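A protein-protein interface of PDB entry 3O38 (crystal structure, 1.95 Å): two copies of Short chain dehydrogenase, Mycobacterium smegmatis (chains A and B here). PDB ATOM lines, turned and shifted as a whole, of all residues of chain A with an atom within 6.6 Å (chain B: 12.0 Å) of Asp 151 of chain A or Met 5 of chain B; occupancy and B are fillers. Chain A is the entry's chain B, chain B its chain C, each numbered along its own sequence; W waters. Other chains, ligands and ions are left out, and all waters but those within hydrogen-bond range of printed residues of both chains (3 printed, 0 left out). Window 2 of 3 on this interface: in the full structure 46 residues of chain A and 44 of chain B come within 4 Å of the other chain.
O of Asp 151 of chain A sits at hydrogen-bond distance from N of Met 5 of chain B, at 2.8 Å.
The backbone NH (N) of Gly 154 of chain A sits at hydrogen-bond distance from the backbone carbonyl oxygen (O) of Gly 196 of chain A.
The guanidinium group (NE) of Arg 232 of chain B is in hydrogen-bond range of the backbone carbonyl oxygen (O) of Leu 7 of chain B (2.8 Å).
The backbone carbonyl oxygen (O) of Pro 11 of chain B lies within hydrogen-bond range of the indole nitrogen (NE1) of Trp 237 of chain B, 3.0 Å away.
Met 5 of chain B touches His 152 of chain A.
Met 5 of chain B touches Gly 153 of chain A.
Val 193 of chain A touches Leu 7 of chain B (CA to CD1, 3.8 Å).
Val 193 of chain A touches Ala 229 of chain B (CG2 to O, 3.5 Å).
Phe 230 of chain B touches Val 193 of chain A.
O of Gly 196 of chain A touches CG of Met 5 of chain B, at 3.7 Å.
C of Gly 196 of chain A touches CD1 of Leu 7 of chain B, at 3.9 Å.
Leu 7 of chain B touches Val 197 of chain A.
CB of Asp 249 of chain A touches CG2 of Ile 14 of chain B (3.7 Å).
Asp 249 of chain A touches Trp 237 of chain B (O to CH2, 3.98 Å).
Of chain B, only Met 5 comes within 4 Å of Asp 151 of chain A.
Met 5 of chain B touches just these residues of chain A: Asp 151, His 152, Gly 153 and Gly 196.
No residue of chain B comes within 4 Å of Gly 149 of chain A.
No residue of chain B comes within 4 Å of Val 150 of chain A.
Of chain B, only Met 5 (3.97 Å) comes within 4 Å of Gly 153 of chain A.
No residue of chain B comes within 4 Å of Gly 154 of chain A.
Printed residues of chain B within 4 Å of Gly 196 of chain A: Met 5 and Leu 7.
Printed residues of chain A within 4 Å of Ile 14 of chain B: Asp 249.
Of the printed residues of chain B, Asp 249 of chain A touches Ile 14 (3.7 Å) and Trp 237 (3.98 Å).
Ser 8 of chain B touches none of the printed residues of chain A.
Lys 12 of chain B touches none of the printed residues of chain A.
The nearest printed residue of chain A that does not touch Ala 229 of chain B is Glu 194 of chain A (6.8 Å).
Of the 14 printed residues of chain A, 7 touch a printed residue of chain B.
Printed residues of chain A that touch a printed residue of chain B: Asp 151, His 152, Gly 153, Val 193, Gly 196, Val 197 and Asp 249.
Printed residues of chain B that touch a printed residue of chain A: Met 5, Leu 7, Ile 14, Ala 229, Phe 230 and Trp 237.
Hydrophobic or aromatic side chains of chain B that line the printed part of chain A: Met 5, Leu 7, Ile 14, Phe 230 and Trp 237.
Along chain B the printed residues that touch a printed residue of chain A span positions 5 to 237.
Among the printed residues, 11 pairs touch across the chains.
Among the printed residues, no Asp or Glu carboxylate lies within 4 Å of a Lys or Arg side-chain nitrogen of the other chain.
No position is printed for both chains.
Water W1 lies within hydrogen-bond range of O of Met 5 of chain B (2.6 Å) and O of Asp 151 of chain A (3.0 Å).
Water W3 lies within hydrogen-bond range of the backbone carbonyl oxygen of Glu 194 of chain A (2.7 Å), the backbone carbonyl oxygen of Met 5 of chain B (3.5 Å) and the backbone NH of Gly 196 of chain A (3.5 Å).
Water W2 bridges O of Val 193 of chain A (2.7 Å) and N of Leu 7 of chain B (2.9 Å).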
ATOM      1  N   PHE A 147     -19.779 -40.970  24.944  1.00  0.00           N
ATOM      2  CA  PHE A 147     -20.165 -39.556  25.012  1.00  0.00           C
ATOM      3  C   PHE A 147     -19.928 -38.951  26.382  1.00  0.00           C
ATOM      4  O   PHE A 147     -19.546 -37.795  26.470  1.00  0.00           O
ATOM      5  CB  PHE A 147     -21.635 -39.299  24.599  1.00  0.00           C
ATOM      6  CG  PHE A 147     -21.892 -39.443  23.114  1.00  0.00           C
ATOM      7  CD1 PHE A 147     -21.193 -38.678  22.185  1.00  0.00           C
ATOM      8  CD2 PHE A 147     -22.835 -40.352  22.656  1.00  0.00           C
ATOM      9  CE1 PHE A 147     -21.445 -38.802  20.785  1.00  0.00           C
ATOM     10  CE2 PHE A 147     -23.099 -40.484  21.276  1.00  0.00           C
ATOM     11  CZ  PHE A 147     -22.384 -39.709  20.340  1.00  0.00           C
ATOM     12  N   ARG A 148     -20.186 -39.718  27.448  1.00  0.00           N
ATOM     13  CA  ARG A 148     -19.850 -39.289  28.824  1.00  0.00           C
ATOM     14  C   ARG A 148     -18.371 -38.867  28.904  1.00  0.00           C
ATOM     15  O   ARG A 148     -18.031 -37.911  29.606  1.00  0.00           O
ATOM     16  CB  ARG A 148     -20.177 -40.411  29.850  1.00  0.00           C
ATOM     17  CG  ARG A 148     -19.886 -40.056  31.339  1.00  0.00           C
ATOM     18  CD  ARG A 148     -20.394 -41.151  32.312  1.00  0.00           C
ATOM     19  NE  ARG A 148     -19.704 -42.426  32.074  1.00  0.00           N
ATOM     20  CZ  ARG A 148     -20.079 -43.611  32.562  1.00  0.00           C
ATOM     21  NH1 ARG A 148     -21.153 -43.708  33.334  1.00  0.00           N
ATOM     22  NH2 ARG A 148     -19.375 -44.699  32.272  1.00  0.00           N
ATOM     23  N   GLY A 149     -17.505 -39.573  28.174  1.00  0.00           N
ATOM     24  CA  GLY A 149     -16.050 -39.321  28.237  1.00  0.00           C
ATOM     25  C   GLY A 149     -15.507 -38.167  27.382  1.00  0.00           C
ATOM     26  O   GLY A 149     -14.307 -37.879  27.431  1.00  0.00           O
ATOM     27  N   VAL A 150     -16.366 -37.506  26.602  1.00  0.00           N
ATOM     28  CA  VAL A 150     -15.934 -36.372  25.770  1.00  0.00           C
ATOM     29  C   VAL A 150     -16.811 -35.148  26.059  1.00  0.00           C
ATOM     30  O   VAL A 150     -17.768 -35.237  26.826  1.00  0.00           O
ATOM     31  CB  VAL A 150     -15.983 -36.692  24.241  1.00  0.00           C
ATOM     32  CG1 VAL A 150     -15.032 -37.831  23.877  1.00  0.00           C
ATOM     33  CG2 VAL A 150     -17.416 -37.044  23.803  1.00  0.00           C
ATOM     34  N   ASP A 151     -16.504 -34.009  25.442  1.00  0.00           N
ATOM     35  CA  ASP A 151     -17.230 -32.799  25.792  1.00  0.00           C
ATOM     36  C   ASP A 151     -18.169 -32.313  24.684  1.00  0.00           C
ATOM     37  O   ASP A 151     -18.928 -31.349  24.888  1.00  0.00           O
ATOM     38  CB  ASP A 151     -16.263 -31.695  26.211  1.00  0.00           C
ATOM     39  CG  ASP A 151     -15.517 -32.035  27.513  1.00  0.00           C
ATOM     40  OD1 ASP A 151     -16.139 -32.516  28.490  1.00  0.00           O
ATOM     41  OD2 ASP A 151     -14.312 -31.804  27.559  1.00  0.00           O
ATOM     42  N   HIS A 152     -18.117 -32.948  23.515  1.00  0.00           N
ATOM     43  CA  HIS A 152     -18.820 -32.365  22.369  1.00  0.00           C
ATOM     44  C   HIS A 152     -20.240 -32.866  22.206  1.00  0.00           C
ATOM     45  O   HIS A 152     -21.002 -32.345  21.358  1.00  0.00           O
ATOM     46  CB  HIS A 152     -18.043 -32.574  21.076  1.00  0.00           C
ATOM     47  CG  HIS A 152     -17.707 -34.004  20.787  1.00  0.00           C
ATOM     48  ND1 HIS A 152     -18.661 -34.953  20.487  1.00  0.00           N
ATOM     49  CD2 HIS A 152     -16.513 -34.629  20.698  1.00  0.00           C
ATOM     50  CE1 HIS A 152     -18.069 -36.114  20.257  1.00  0.00           C
ATOM     51  NE2 HIS A 152     -16.762 -35.941  20.382  1.00  0.00           N
ATOM     52  N   GLY A 153     -20.587 -33.909  22.950  1.00  0.00           N
ATOM     53  CA  GLY A 153     -21.948 -34.437  22.920  1.00  0.00           C
ATOM     54  C   GLY A 153     -22.233 -35.071  21.554  1.00  0.00           C
ATOM     55  O   GLY A 153     -21.299 -35.345  20.769  1.00  0.00           O
ATOM     56  N   GLY A 154     -23.511 -35.309  21.279  1.00  0.00           N
ATOM     57  CA  GLY A 154     -23.909 -36.011  20.049  1.00  0.00           C
ATOM     58  C   GLY A 154     -25.381 -36.360  19.965  1.00  0.00           C
ATOM     59  O   GLY A 154     -26.218 -35.861  20.718  1.00  0.00           O
ATOM     60  N   VAL A 193     -29.210 -36.384  28.387  1.00  0.00           N
ATOM     61  CA  VAL A 193     -29.029 -34.943  28.540  1.00  0.00           C
ATOM     62  C   VAL A 193     -27.724 -34.620  29.275  1.00  0.00           C
ATOM     63  O   VAL A 193     -27.010 -33.715  28.865  1.00  0.00           O
ATOM     64  CB  VAL A 193     -30.239 -34.276  29.279  1.00  0.00           C
ATOM     65  CG1 VAL A 193     -30.011 -32.754  29.533  1.00  0.00           C
ATOM     66  CG2 VAL A 193     -31.507 -34.472  28.463  1.00  0.00           C
ATOM     67  N   GLU A 194     -27.421 -35.387  30.332  1.00  0.00           N
ATOM     68  CA  GLU A 194     -26.195 -35.215  31.144  1.00  0.00           C
ATOM     69  C   GLU A 194     -24.928 -35.210  30.267  1.00  0.00           C
ATOM     70  O   GLU A 194     -24.004 -34.444  30.510  1.00  0.00           O
ATOM     71  CB  GLU A 194     -26.105 -36.335  32.201  1.00  0.00           C
ATOM     72  CG  GLU A 194     -25.164 -35.969  33.385  1.00  0.00           C
ATOM     73  CD  GLU A 194     -25.110 -37.037  34.480  1.00  0.00           C
ATOM     74  OE1 GLU A 194     -25.947 -37.956  34.499  1.00  0.00           O
ATOM     75  OE2 GLU A 194     -24.222 -36.944  35.340  1.00  0.00           O
ATOM     76  N   PHE A 195     -24.897 -36.067  29.245  1.00  0.00           N
ATOM     77  CA  PHE A 195     -23.728 -36.207  28.365  1.00  0.00           C
ATOM     78  C   PHE A 195     -23.772 -35.388  27.069  1.00  0.00           C
ATOM     79  O   PHE A 195     -22.906 -35.529  26.201  1.00  0.00           O
ATOM     80  CB  PHE A 195     -23.432 -37.699  28.125  1.00  0.00           C
ATOM     81  CG  PHE A 195     -23.663 -38.562  29.362  1.00  0.00           C
ATOM     82  CD1 PHE A 195     -23.084 -38.225  30.577  1.00  0.00           C
ATOM     83  CD2 PHE A 195     -24.494 -39.679  29.312  1.00  0.00           C
ATOM     84  CE1 PHE A 195     -23.304 -39.003  31.727  1.00  0.00           C
ATOM     85  CE2 PHE A 195     -24.732 -40.457  30.444  1.00  0.00           C
ATOM     86  CZ  PHE A 195     -24.146 -40.115  31.650  1.00  0.00           C
ATOM     87  N   GLY A 196     -24.752 -34.495  26.970  1.00  0.00           N
ATOM     88  CA  GLY A 196     -24.854 -33.614  25.808  1.00  0.00           C
ATOM     89  C   GLY A 196     -25.385 -34.382  24.606  1.00  0.00           C
ATOM     90  O   GLY A 196     -25.147 -34.005  23.477  1.00  0.00           O
ATOM     91  N   VAL A 197     -26.127 -35.452  24.857  1.00  0.00           N
ATOM     92  CA  VAL A 197     -26.658 -36.290  23.785  1.00  0.00           C
ATOM     93  C   VAL A 197     -28.197 -36.172  23.678  1.00  0.00           C
ATOM     94  O   VAL A 197     -28.913 -36.195  24.699  1.00  0.00           O
ATOM     95  CB  VAL A 197     -26.190 -37.749  23.976  1.00  0.00           C
ATOM     96  CG1 VAL A 197     -26.802 -38.704  22.927  1.00  0.00           C
ATOM     97  CG2 VAL A 197     -24.652 -37.815  23.903  1.00  0.00           C
ATOM     98  N   ASP A 249     -28.991 -30.381  13.356  1.00  0.00           N
ATOM     99  CA  ASP A 249     -29.383 -29.285  14.255  1.00  0.00           C
ATOM    100  C   ASP A 249     -30.802 -28.728  14.027  1.00  0.00           C
ATOM    101  O   ASP A 249     -31.287 -27.896  14.820  1.00  0.00           O
ATOM    102  CB  ASP A 249     -28.381 -28.142  14.143  1.00  0.00           C
ATOM    103  CG  ASP A 249     -27.028 -28.491  14.717  1.00  0.00           C
ATOM    104  OD1 ASP A 249     -26.946 -29.491  15.460  1.00  0.00           O
ATOM    105  OD2 ASP A 249     -26.048 -27.790  14.377  1.00  0.00           O
ATOM    106  N   MET B   5     -20.399 -28.942  24.570  1.00  0.00           N
ATOM    107  CA  MET B   5     -21.876 -29.114  24.451  1.00  0.00           C
ATOM    108  C   MET B   5     -22.502 -29.224  25.831  1.00  0.00           C
ATOM    109  O   MET B   5     -22.153 -30.117  26.612  1.00  0.00           O
ATOM    110  CB  MET B   5     -22.233 -30.358  23.631  1.00  0.00           C
ATOM    111  CG  MET B   5     -23.738 -30.616  23.493  1.00  0.00           C
ATOM    112  SD  MET B   5     -24.733 -29.121  23.133  1.00  0.00           S
ATOM    113  CE  MET B   5     -24.519 -28.944  21.366  1.00  0.00           C
ATOM    114  N   ASN B   6     -23.441 -28.318  26.104  1.00  0.00           N
ATOM    115  CA  ASN B   6     -24.238 -28.301  27.330  1.00  0.00           C
ATOM    116  C   ASN B   6     -25.682 -27.939  26.990  1.00  0.00           C
ATOM    117  O   ASN B   6     -25.968 -26.800  26.615  1.00  0.00           O
ATOM    118  CB  ASN B   6     -23.674 -27.281  28.327  1.00  0.00           C
ATOM    119  CG  ASN B   6     -24.521 -27.148  29.573  1.00  0.00           C
ATOM    120  OD1 ASN B   6     -25.621 -27.711  29.677  1.00  0.00           O
ATOM    121  ND2 ASN B   6     -24.013 -26.406  30.539  1.00  0.00           N
ATOM    122  N   LEU B   7     -26.592 -28.901  27.162  1.00  0.00           N
ATOM    123  CA  LEU B   7     -27.958 -28.750  26.628  1.00  0.00           C
ATOM    124  C   LEU B   7     -28.863 -27.729  27.345  1.00  0.00           C
ATOM    125  O   LEU B   7     -29.889 -27.316  26.782  1.00  0.00           O
ATOM    126  CB  LEU B   7     -28.649 -30.114  26.426  1.00  0.00           C
ATOM    127  CG  LEU B   7     -28.018 -31.124  25.454  1.00  0.00           C
ATOM    128  CD1 LEU B   7     -28.668 -32.520  25.592  1.00  0.00           C
ATOM    129  CD2 LEU B   7     -28.094 -30.616  23.980  1.00  0.00           C
ATOM    130  N   SER B   8     -28.487 -27.286  28.540  1.00  0.00           N
ATOM    131  CA  SER B   8     -29.250 -26.242  29.226  1.00  0.00           C
ATOM    132  C   SER B   8     -28.891 -24.827  28.738  1.00  0.00           C
ATOM    133  O   SER B   8     -29.540 -23.839  29.095  1.00  0.00           O
ATOM    134  CB  SER B   8     -29.064 -26.331  30.732  1.00  0.00           C
ATOM    135  OG  SER B   8     -27.788 -25.813  31.107  1.00  0.00           O
ATOM    136  N   GLU B   9     -27.835 -24.725  27.945  1.00  0.00           N
ATOM    137  CA  GLU B   9     -27.464 -23.447  27.370  1.00  0.00           C
ATOM    138  C   GLU B   9     -28.275 -23.209  26.098  1.00  0.00           C
ATOM    139  O   GLU B   9     -28.462 -24.115  25.300  1.00  0.00           O
ATOM    140  CB  GLU B   9     -25.959 -23.387  27.089  1.00  0.00           C
ATOM    141  CG  GLU B   9     -25.094 -23.518  28.361  1.00  0.00           C
ATOM    142  CD  GLU B   9     -23.602 -23.733  28.067  1.00  0.00           C
ATOM    143  OE1 GLU B   9     -23.196 -23.764  26.866  1.00  0.00           O
ATOM    144  OE2 GLU B   9     -22.841 -23.891  29.048  1.00  0.00           O
ATOM    145  N   ALA B  10     -28.759 -21.985  25.934  1.00  0.00           N
ATOM    146  CA  ALA B  10     -29.543 -21.605  24.767  1.00  0.00           C
ATOM    147  C   ALA B  10     -28.627 -21.645  23.528  1.00  0.00           C
ATOM    148  O   ALA B  10     -27.631 -20.954  23.501  1.00  0.00           O
ATOM    149  CB  ALA B  10     -30.125 -20.200  24.998  1.00  0.00           C
ATOM    150  N   PRO B  11     -28.931 -22.495  22.522  1.00  0.00           N
ATOM    151  CA  PRO B  11     -28.002 -22.621  21.387  1.00  0.00           C
ATOM    152  C   PRO B  11     -28.139 -21.476  20.378  1.00  0.00           C
ATOM    153  O   PRO B  11     -29.194 -20.815  20.328  1.00  0.00           O
ATOM    154  CB  PRO B  11     -28.425 -23.944  20.725  1.00  0.00           C
ATOM    155  CG  PRO B  11     -29.855 -24.123  21.098  1.00  0.00           C
ATOM    156  CD  PRO B  11     -30.042 -23.466  22.445  1.00  0.00           C
ATOM    157  N   LYS B  12     -27.087 -21.251  19.581  1.00  0.00           N
ATOM    158  CA  LYS B  12     -27.124 -20.196  18.559  1.00  0.00           C
ATOM    159  C   LYS B  12     -27.930 -20.651  17.351  1.00  0.00           C
ATOM    160  O   LYS B  12     -27.794 -21.782  16.890  1.00  0.00           O
ATOM    161  CB  LYS B  12     -25.715 -19.792  18.102  1.00  0.00           C
ATOM    162  N   GLU B  13     -28.760 -19.756  16.831  1.00  0.00           N
ATOM    163  CA  GLU B  13     -29.494 -20.026  15.611  1.00  0.00           C
ATOM    164  C   GLU B  13     -28.548 -20.508  14.503  1.00  0.00           C
ATOM    165  O   GLU B  13     -27.521 -19.869  14.245  1.00  0.00           O
ATOM    166  CB  GLU B  13     -30.287 -18.785  15.179  1.00  0.00           C
ATOM    167  CG  GLU B  13     -31.184 -19.039  13.970  1.00  0.00           C
ATOM    168  CD  GLU B  13     -32.124 -17.886  13.665  1.00  0.00           C
ATOM    169  OE1 GLU B  13     -31.965 -16.804  14.248  1.00  0.00           O
ATOM    170  OE2 GLU B  13     -33.032 -18.062  12.846  1.00  0.00           O
ATOM    171  N   ILE B  14     -28.884 -21.639  13.879  1.00  0.00           N
ATOM    172  CA  ILE B  14     -28.072 -22.213  12.789  1.00  0.00           C
ATOM    173  C   ILE B  14     -28.260 -21.481  11.459  1.00  0.00           C
ATOM    174  O   ILE B  14     -29.312 -20.865  11.224  1.00  0.00           O
ATOM    175  CB  ILE B  14     -28.335 -23.743  12.613  1.00  0.00           C
ATOM    176  CG1 ILE B  14     -29.787 -24.011  12.144  1.00  0.00           C
ATOM    177  CG2 ILE B  14     -27.934 -24.505  13.907  1.00  0.00           C
ATOM    178  CD1 ILE B  14     -30.168 -25.530  11.962  1.00  0.00           C
ATOM    179  N   ALA B 229     -36.828 -31.535  29.616  1.00  0.00           N
ATOM    180  CA  ALA B 229     -35.689 -32.463  29.554  1.00  0.00           C
ATOM    181  C   ALA B 229     -34.323 -31.762  29.613  1.00  0.00           C
ATOM    182  O   ALA B 229     -33.415 -32.218  30.329  1.00  0.00           O
ATOM    183  CB  ALA B 229     -35.790 -33.347  28.289  1.00  0.00           C
ATOM    184  N   PHE B 230     -34.165 -30.654  28.885  1.00  0.00           N
ATOM    185  CA  PHE B 230     -32.874 -29.953  28.858  1.00  0.00           C
ATOM    186  C   PHE B 230     -32.744 -28.943  30.001  1.00  0.00           C
ATOM    187  O   PHE B 230     -31.695 -28.343  30.159  1.00  0.00           O
ATOM    188  CB  PHE B 230     -32.640 -29.181  27.562  1.00  0.00           C
ATOM    189  CG  PHE B 230     -32.573 -30.017  26.311  1.00  0.00           C
ATOM    190  CD1 PHE B 230     -32.430 -31.401  26.353  1.00  0.00           C
ATOM    191  CD2 PHE B 230     -32.619 -29.391  25.067  1.00  0.00           C
ATOM    192  CE1 PHE B 230     -32.377 -32.156  25.157  1.00  0.00           C
ATOM    193  CE2 PHE B 230     -32.562 -30.144  23.859  1.00  0.00           C
ATOM    194  CZ  PHE B 230     -32.429 -31.538  23.929  1.00  0.00           C
ATOM    195  N   GLY B 231     -33.818 -28.728  30.764  1.00  0.00           N
ATOM    196  CA  GLY B 231     -33.804 -27.682  31.808  1.00  0.00           C
ATOM    197  C   GLY B 231     -33.757 -26.270  31.238  1.00  0.00           C
ATOM    198  O   GLY B 231     -33.276 -25.338  31.897  1.00  0.00           O
ATOM    199  N   ARG B 232     -34.253 -26.099  30.014  1.00  0.00           N
ATOM    200  CA  ARG B 232     -34.394 -24.767  29.411  1.00  0.00           C
ATOM    201  C   ARG B 232     -35.600 -24.808  28.492  1.00  0.00           C
ATOM    202  O   ARG B 232     -35.989 -25.896  28.035  1.00  0.00           O
ATOM    203  CB  ARG B 232     -33.113 -24.358  28.633  1.00  0.00           C
ATOM    204  CG  ARG B 232     -32.818 -25.219  27.400  1.00  0.00           C
ATOM    205  CD  ARG B 232     -31.708 -24.703  26.479  1.00  0.00           C
ATOM    206  NE  ARG B 232     -31.514 -25.598  25.309  1.00  0.00           N
ATOM    207  CZ  ARG B 232     -32.178 -25.534  24.154  1.00  0.00           C
ATOM    208  NH1 ARG B 232     -33.088 -24.584  23.941  1.00  0.00           N
ATOM    209  NH2 ARG B 232     -31.918 -26.413  23.174  1.00  0.00           N
ATOM    210  N   GLU B 235     -35.779 -22.219  22.169  1.00  0.00           N
ATOM    211  CA  GLU B 235     -35.635 -20.944  21.473  1.00  0.00           C
ATOM    212  C   GLU B 235     -36.675 -20.873  20.355  1.00  0.00           C
ATOM    213  O   GLU B 235     -36.933 -21.873  19.675  1.00  0.00           O
ATOM    214  CB  GLU B 235     -34.220 -20.810  20.917  1.00  0.00           C
ATOM    215  CG  GLU B 235     -33.170 -20.752  21.988  1.00  0.00           C
ATOM    216  CD  GLU B 235     -33.241 -19.452  22.816  1.00  0.00           C
ATOM    217  OE1 GLU B 235     -32.706 -18.436  22.330  1.00  0.00           O
ATOM    218  OE2 GLU B 235     -33.789 -19.456  23.940  1.00  0.00           O
ATOM    219  N   TRP B 237     -36.243 -19.958  17.539  1.00  0.00           N
ATOM    220  CA  TRP B 237     -35.589 -20.423  16.304  1.00  0.00           C
ATOM    221  C   TRP B 237     -35.647 -21.949  16.200  1.00  0.00           C
ATOM    222  O   TRP B 237     -35.749 -22.473  15.114  1.00  0.00           O
ATOM    223  CB  TRP B 237     -34.146 -19.923  16.119  1.00  0.00           C
ATOM    224  CG  TRP B 237     -33.046 -20.677  16.860  1.00  0.00           C
ATOM    225  CD1 TRP B 237     -32.407 -20.270  18.001  1.00  0.00           C
ATOM    226  CD2 TRP B 237     -32.429 -21.934  16.484  1.00  0.00           C
ATOM    227  NE1 TRP B 237     -31.444 -21.195  18.355  1.00  0.00           N
ATOM    228  CE2 TRP B 237     -31.441 -22.222  17.448  1.00  0.00           C
ATOM    229  CE3 TRP B 237     -32.625 -22.841  15.431  1.00  0.00           C
ATOM    230  CZ2 TRP B 237     -30.647 -23.387  17.396  1.00  0.00           C
ATOM    231  CZ3 TRP B 237     -31.833 -23.980  15.370  1.00  0.00           C
ATOM    232  CH2 TRP B 237     -30.863 -24.251  16.352  1.00  0.00           C
ATOM    233  N   GLU B 238     -35.633 -22.644  17.336  1.00  0.00           N
ATOM    234  CA  GLU B 238     -35.673 -24.119  17.305  1.00  0.00           C
ATOM    235  C   GLU B 238     -37.014 -24.654  16.802  1.00  0.00           C
ATOM    236  O   GLU B 238     -37.047 -25.618  16.023  1.00  0.00           O
ATOM    237  CB  GLU B 238     -35.307 -24.717  18.668  1.00  0.00           C
ATOM    238  CG  GLU B 238     -33.872 -24.453  19.101  1.00  0.00           C
ATOM    239  CD  GLU B 238     -33.583 -24.940  20.509  1.00  0.00           C
ATOM    240  OE1 GLU B 238     -34.076 -24.316  21.475  1.00  0.00           O
ATOM    241  OE2 GLU B 238     -32.856 -25.953  20.665  1.00  0.00           O
HETATM  242  O   HOH W   1     -20.920 -32.405  26.924  1.00  0.00           O
HETATM  243  O   HOH W   2     -25.823 -31.284  28.616  1.00  0.00           O
HETATM  244  O   HOH W   3     -23.046 -32.349  29.122  1.00  0.00           O
